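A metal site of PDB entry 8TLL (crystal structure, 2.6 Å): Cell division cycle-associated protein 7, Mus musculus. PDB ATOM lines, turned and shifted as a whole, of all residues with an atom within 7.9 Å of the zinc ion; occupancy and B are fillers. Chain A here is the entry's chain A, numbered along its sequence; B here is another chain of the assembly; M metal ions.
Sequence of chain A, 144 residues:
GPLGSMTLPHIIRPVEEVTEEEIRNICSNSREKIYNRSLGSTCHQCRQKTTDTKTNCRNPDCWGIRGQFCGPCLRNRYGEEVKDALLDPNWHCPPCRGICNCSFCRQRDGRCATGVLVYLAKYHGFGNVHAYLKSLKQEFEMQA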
ATOM      1  N   SER A  30      20.907  23.684  25.958  1.00  0.00           N
ATOM      2  CA  SER A  30      19.653  24.020  25.298  1.00  0.00           C
ATOM      3  C   SER A  30      19.574  23.456  23.881  1.00  0.00           C
ATOM      4  O   SER A  30      18.534  22.939  23.465  1.00  0.00           O
ATOM      5  CB  SER A  30      19.474  25.547  25.278  1.00  0.00           C
ATOM      6  OG  SER A  30      18.356  25.917  24.488  1.00  0.00           O
ATOM      7  N   LYS A  33      18.285  19.567  22.771  1.00  0.00           N
ATOM      8  CA  LYS A  33      16.942  19.174  23.163  1.00  0.00           C
ATOM      9  C   LYS A  33      16.278  18.355  22.062  1.00  0.00           C
ATOM     10  O   LYS A  33      16.609  18.461  20.880  1.00  0.00           O
ATOM     11  CB  LYS A  33      16.090  20.390  23.498  1.00  0.00           C
ATOM     12  CG  LYS A  33      16.393  21.018  24.847  1.00  0.00           C
ATOM     13  CD  LYS A  33      15.385  22.106  25.159  1.00  0.00           C
ATOM     14  CE  LYS A  33      15.513  22.583  26.587  1.00  0.00           C
ATOM     15  NZ  LYS A  33      14.587  23.717  26.841  1.00  0.00           N
ATOM     16  N   THR A  42       6.310  21.279  27.889  1.00  0.00           N
ATOM     17  CA  THR A  42       6.691  22.656  27.599  1.00  0.00           C
ATOM     18  C   THR A  42       7.311  23.288  28.841  1.00  0.00           C
ATOM     19  O   THR A  42       6.782  23.142  29.943  1.00  0.00           O
ATOM     20  CB  THR A  42       5.480  23.460  27.132  1.00  0.00           C
ATOM     21  OG1 THR A  42       4.913  22.841  25.974  1.00  0.00           O
ATOM     22  CG2 THR A  42       5.897  24.874  26.763  1.00  0.00           C
ATOM     23  N   CYS A  43       8.449  23.954  28.641  1.00  0.00           N
ATOM     24  CA  CYS A  43       9.041  24.797  29.667  1.00  0.00           C
ATOM     25  C   CYS A  43       8.349  26.152  29.657  1.00  0.00           C
ATOM     26  O   CYS A  43       8.193  26.760  28.602  1.00  0.00           O
ATOM     27  CB  CYS A  43      10.543  24.951  29.405  1.00  0.00           C
ATOM     28  SG  CYS A  43      11.398  26.288  30.288  1.00  0.00           S
ATOM     29  N   HIS A  44       7.915  26.610  30.829  1.00  0.00           N
ATOM     30  CA  HIS A  44       7.205  27.885  30.898  1.00  0.00           C
ATOM     31  C   HIS A  44       8.082  29.042  30.442  1.00  0.00           C
ATOM     32  O   HIS A  44       7.585  29.995  29.831  1.00  0.00           O
ATOM     33  CB  HIS A  44       6.700  28.140  32.328  1.00  0.00           C
ATOM     34  CG  HIS A  44       6.278  29.554  32.579  1.00  0.00           C
ATOM     35  ND1 HIS A  44       5.176  30.129  31.985  1.00  0.00           N
ATOM     36  CD2 HIS A  44       6.803  30.512  33.387  1.00  0.00           C
ATOM     37  CE1 HIS A  44       5.041  31.370  32.406  1.00  0.00           C
ATOM     38  NE2 HIS A  44       6.029  31.631  33.249  1.00  0.00           N
ATOM     39  N   GLN A  45       9.389  28.960  30.697  1.00  0.00           N
ATOM     40  CA  GLN A  45      10.277  30.077  30.394  1.00  0.00           C
ATOM     41  C   GLN A  45      10.594  30.153  28.900  1.00  0.00           C
ATOM     42  O   GLN A  45      10.270  31.136  28.243  1.00  0.00           O
ATOM     43  CB  GLN A  45      11.560  29.961  31.237  1.00  0.00           C
ATOM     44  CG  GLN A  45      12.504  31.145  31.109  1.00  0.00           C
ATOM     45  CD  GLN A  45      12.174  32.284  32.071  1.00  0.00           C
ATOM     46  OE1 GLN A  45      11.466  32.093  33.070  1.00  0.00           O
ATOM     47  NE2 GLN A  45      12.686  33.470  31.772  1.00  0.00           N
ATOM     48  N   CYS A  46      11.217  29.106  28.351  1.00  0.00           N
ATOM     49  CA  CYS A  46      11.618  29.158  26.944  1.00  0.00           C
ATOM     50  C   CYS A  46      10.510  28.742  25.984  1.00  0.00           C
ATOM     51  O   CYS A  46      10.671  28.912  24.777  1.00  0.00           O
ATOM     52  CB  CYS A  46      12.840  28.276  26.695  1.00  0.00           C
ATOM     53  SG  CYS A  46      12.534  26.518  26.879  1.00  0.00           S
ATOM     54  N   ARG A  47       9.399  28.215  26.493  1.00  0.00           N
ATOM     55  CA  ARG A  47       8.228  27.857  25.691  1.00  0.00           C
ATOM     56  C   ARG A  47       8.590  26.867  24.576  1.00  0.00           C
ATOM     57  O   ARG A  47       8.116  26.964  23.450  1.00  0.00           O
ATOM     58  CB  ARG A  47       7.554  29.113  25.129  1.00  0.00           C
ATOM     59  CG  ARG A  47       7.071  30.051  26.236  1.00  0.00           C
ATOM     60  CD  ARG A  47       6.223  31.202  25.723  1.00  0.00           C
ATOM     61  NE  ARG A  47       6.953  32.125  24.864  1.00  0.00           N
ATOM     62  CZ  ARG A  47       7.569  33.214  25.279  1.00  0.00           C
ATOM     63  NH1 ARG A  47       7.607  33.539  26.571  1.00  0.00           N
ATOM     64  NH2 ARG A  47       8.175  34.008  24.401  1.00  0.00           N
ATOM     65  N   GLN A  48       9.437  25.900  24.919  1.00  0.00           N
ATOM     66  CA  GLN A  48       9.784  24.798  24.028  1.00  0.00           C
ATOM     67  C   GLN A  48       9.234  23.510  24.602  1.00  0.00           C
ATOM     68  O   GLN A  48       9.432  23.212  25.790  1.00  0.00           O
ATOM     69  CB  GLN A  48      11.298  24.694  23.834  1.00  0.00           C
ATOM     70  CG  GLN A  48      11.973  25.961  23.319  1.00  0.00           C
ATOM     71  CD  GLN A  48      11.450  26.413  21.957  1.00  0.00           C
ATOM     72  OE1 GLN A  48      11.918  25.957  20.918  1.00  0.00           O
ATOM     73  NE2 GLN A  48      10.466  27.312  21.970  1.00  0.00           N
ATOM     74  N   THR A  50       9.685  19.890  24.778  1.00  0.00           N
ATOM     75  CA  THR A  50      10.706  18.881  24.585  1.00  0.00           C
ATOM     76  C   THR A  50      10.556  17.782  25.629  1.00  0.00           C
ATOM     77  O   THR A  50       9.767  17.894  26.569  1.00  0.00           O
ATOM     78  CB  THR A  50      12.118  19.477  24.652  1.00  0.00           C
ATOM     79  OG1 THR A  50      12.320  20.066  25.943  1.00  0.00           O
ATOM     80  CG2 THR A  50      12.305  20.535  23.574  1.00  0.00           C
ATOM     81  N   ASP A  52      12.935  16.551  27.701  1.00  0.00           N
ATOM     82  CA  ASP A  52      13.805  16.610  28.867  1.00  0.00           C
ATOM     83  C   ASP A  52      12.993  16.828  30.138  1.00  0.00           C
ATOM     84  O   ASP A  52      11.960  17.504  30.140  1.00  0.00           O
ATOM     85  CB  ASP A  52      14.822  17.733  28.697  1.00  0.00           C
ATOM     86  CG  ASP A  52      14.176  19.057  28.344  1.00  0.00           C
ATOM     87  OD1 ASP A  52      13.723  19.761  29.277  1.00  0.00           O
ATOM     88  OD2 ASP A  52      14.100  19.380  27.147  1.00  0.00           O
ATOM     89  N   LYS A  54      11.502  18.152  33.467  1.00  0.00           N
ATOM     90  CA  LYS A  54      11.248  19.518  33.894  1.00  0.00           C
ATOM     91  C   LYS A  54      10.698  19.525  35.310  1.00  0.00           C
ATOM     92  O   LYS A  54      10.232  18.499  35.816  1.00  0.00           O
ATOM     93  CB  LYS A  54      10.305  20.240  32.923  1.00  0.00           C
ATOM     94  CG  LYS A  54      10.906  20.387  31.547  1.00  0.00           C
ATOM     95  CD  LYS A  54       9.959  21.031  30.564  1.00  0.00           C
ATOM     96  CE  LYS A  54      10.629  21.192  29.226  1.00  0.00           C
ATOM     97  NZ  LYS A  54      10.990  19.876  28.641  1.00  0.00           N
ATOM     98  N   GLN A  68       6.578  24.291  35.112  1.00  0.00           N
ATOM     99  CA  GLN A  68       7.515  23.422  34.421  1.00  0.00           C
ATOM    100  C   GLN A  68       8.624  24.251  33.789  1.00  0.00           C
ATOM    101  O   GLN A  68       8.353  25.084  32.929  1.00  0.00           O
ATOM    102  CB  GLN A  68       6.815  22.583  33.351  1.00  0.00           C
ATOM    103  CG  GLN A  68       5.858  21.557  33.878  1.00  0.00           C
ATOM    104  CD  GLN A  68       5.157  20.832  32.748  1.00  0.00           C
ATOM    105  OE1 GLN A  68       5.407  21.117  31.584  1.00  0.00           O
ATOM    106  NE2 GLN A  68       4.267  19.908  33.097  1.00  0.00           N
ATOM    107  N   PHE A  69       9.856  23.985  34.196  1.00  0.00           N
ATOM    108  CA  PHE A  69      11.024  24.695  33.697  1.00  0.00           C
ATOM    109  C   PHE A  69      12.064  23.679  33.256  1.00  0.00           C
ATOM    110  O   PHE A  69      12.275  22.664  33.929  1.00  0.00           O
ATOM    111  CB  PHE A  69      11.613  25.619  34.773  1.00  0.00           C
ATOM    112  CG  PHE A  69      10.778  26.841  35.031  1.00  0.00           C
ATOM    113  CD1 PHE A  69       9.652  26.778  35.832  1.00  0.00           C
ATOM    114  CD2 PHE A  69      11.130  28.058  34.465  1.00  0.00           C
ATOM    115  CE1 PHE A  69       8.890  27.900  36.072  1.00  0.00           C
ATOM    116  CE2 PHE A  69      10.371  29.193  34.702  1.00  0.00           C
ATOM    117  CZ  PHE A  69       9.248  29.106  35.500  1.00  0.00           C
ATOM    118  N   CYS A  70      12.702  23.953  32.124  1.00  0.00           N
ATOM    119  CA  CYS A  70      13.759  23.075  31.650  1.00  0.00           C
ATOM    120  C   CYS A  70      15.051  23.324  32.422  1.00  0.00           C
ATOM    121  O   CYS A  70      15.177  24.291  33.184  1.00  0.00           O
ATOM    122  CB  CYS A  70      13.986  23.268  30.159  1.00  0.00           C
ATOM    123  SG  CYS A  70      14.672  24.871  29.695  1.00  0.00           S
ATOM    124  N   GLY A  71      16.011  22.424  32.230  1.00  0.00           N
ATOM    125  CA  GLY A  71      17.294  22.502  32.885  1.00  0.00           C
ATOM    126  C   GLY A  71      18.001  23.823  32.676  1.00  0.00           C
ATOM    127  O   GLY A  71      18.308  24.544  33.624  1.00  0.00           O
ATOM    128  N   PRO A  72      18.290  24.161  31.407  1.00  0.00           N
ATOM    129  CA  PRO A  72      18.959  25.441  31.146  1.00  0.00           C
ATOM    130  C   PRO A  72      18.204  26.649  31.674  1.00  0.00           C
ATOM    131  O   PRO A  72      18.833  27.592  32.155  1.00  0.00           O
ATOM    132  CB  PRO A  72      19.055  25.457  29.617  1.00  0.00           C
ATOM    133  CG  PRO A  72      19.137  24.026  29.251  1.00  0.00           C
ATOM    134  CD  PRO A  72      18.210  23.331  30.193  1.00  0.00           C
ATOM    135  N   CYS A  73      16.867  26.645  31.609  1.00  0.00           N
ATOM    136  CA  CYS A  73      16.130  27.859  31.943  1.00  0.00           C
ATOM    137  C   CYS A  73      16.179  28.163  33.434  1.00  0.00           C
ATOM    138  O   CYS A  73      16.381  29.317  33.824  1.00  0.00           O
ATOM    139  CB  CYS A  73      14.683  27.745  31.472  1.00  0.00           C
ATOM    140  SG  CYS A  73      14.446  28.334  29.775  1.00  0.00           S
ATOM    141  N   LEU A  74      16.027  27.146  34.293  1.00  0.00           N
ATOM    142  CA  LEU A  74      16.010  27.386  35.727  1.00  0.00           C
ATOM    143  C   LEU A  74      17.374  27.842  36.232  1.00  0.00           C
ATOM    144  O   LEU A  74      17.454  28.690  37.129  1.00  0.00           O
ATOM    145  CB  LEU A  74      15.559  26.137  36.475  1.00  0.00           C
ATOM    146  CG  LEU A  74      15.073  26.387  37.904  1.00  0.00           C
ATOM    147  CD1 LEU A  74      13.813  27.214  37.892  1.00  0.00           C
ATOM    148  CD2 LEU A  74      14.840  25.069  38.619  1.00  0.00           C
ATOM    149  N   ARG A  77      18.025  31.636  34.323  1.00  0.00           N
ATOM    150  CA  ARG A  77      17.123  32.717  34.665  1.00  0.00           C
ATOM    151  C   ARG A  77      16.854  32.837  36.155  1.00  0.00           C
ATOM    152  O   ARG A  77      16.357  33.878  36.606  1.00  0.00           O
ATOM    153  CB  ARG A  77      15.790  32.534  33.930  1.00  0.00           C
ATOM    154  CG  ARG A  77      15.947  32.250  32.448  1.00  0.00           C
ATOM    155  CD  ARG A  77      16.597  33.420  31.731  1.00  0.00           C
ATOM    156  NE  ARG A  77      15.739  34.598  31.761  1.00  0.00           N
ATOM    157  CZ  ARG A  77      15.957  35.692  31.037  1.00  0.00           C
ATOM    158  NH1 ARG A  77      16.991  35.802  30.232  1.00  0.00           N
ATOM    159  NH2 ARG A  77      15.097  36.706  31.131  1.00  0.00           N
ATOM    160  P    DT B   8      18.731  32.600  28.266  1.00  0.00           P
ATOM    161  OP1  DT B   8      18.961  33.681  29.237  1.00  0.00           O
ATOM    162  OP2  DT B   8      18.136  31.330  28.740  1.00  0.00           O
ATOM    163  O5'  DT B   8      17.814  33.153  27.079  1.00  0.00           O
ATOM    164  C5'  DT B   8      17.933  34.501  26.651  1.00  0.00           C
ATOM    165  C4'  DT B   8      16.979  34.781  25.506  1.00  0.00           C
ATOM    166  O4'  DT B   8      17.103  33.727  24.528  1.00  0.00           O
ATOM    167  C3'  DT B   8      15.501  34.778  25.886  1.00  0.00           C
ATOM    168  O3'  DT B   8      15.102  36.088  26.288  1.00  0.00           O
ATOM    169  C2'  DT B   8      14.820  34.375  24.589  1.00  0.00           C
ATOM    170  C1'  DT B   8      15.882  33.551  23.855  1.00  0.00           C
ATOM    171  N1   DT B   8      15.563  32.096  23.787  1.00  0.00           N
ATOM    172  C2   DT B   8      14.698  31.658  22.803  1.00  0.00           C
ATOM    173  O2   DT B   8      14.197  32.408  21.987  1.00  0.00           O
ATOM    174  N3   DT B   8      14.470  30.310  22.809  1.00  0.00           N
ATOM    175  C4   DT B   8      14.986  29.381  23.682  1.00  0.00           C
ATOM    176  O4   DT B   8      14.713  28.190  23.602  1.00  0.00           O
ATOM    177  C5   DT B   8      15.878  29.907  24.687  1.00  0.00           C
ATOM    178  C7   DT B   8      16.500  28.981  25.690  1.00  0.00           C
ATOM    179  C6   DT B   8      16.118  31.218  24.695  1.00  0.00           C
HETATM  180 ZN    ZN M   1      13.258  26.490  28.999  1.00  0.00          ZN
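Merely in contact with the zinc ion: Lys 33 (3.8 Å). Along chain A the residues within 4 Å of the zinc ion span positions 33 to 73.
The zinc ion is bound by SG of Cys 46. The zinc ion is bound by SG of Cys 70 (2.3 Å). The zinc ion is bound by SG of Cys 43 (2.3 Å). The zinc ion is bound by SG of Cys 73 (2.3 Å).
NZ of Lys 33 sits close to SG of Cys 46, at 3.5 Å. O of Cys 46 is in hydrogen-bond range of NE2 of Gln 48. The side-chain sulfur (SG) of Cys 70 lies close to the side-chain amino group (NZ) of Lys 33. SG of Cys 43 lies close to N of Gln 45 (3.4 Å). The backbone NH (N) of Cys 43 is in hydrogen-bond range of the backbone carbonyl oxygen (O) of Gln 48.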
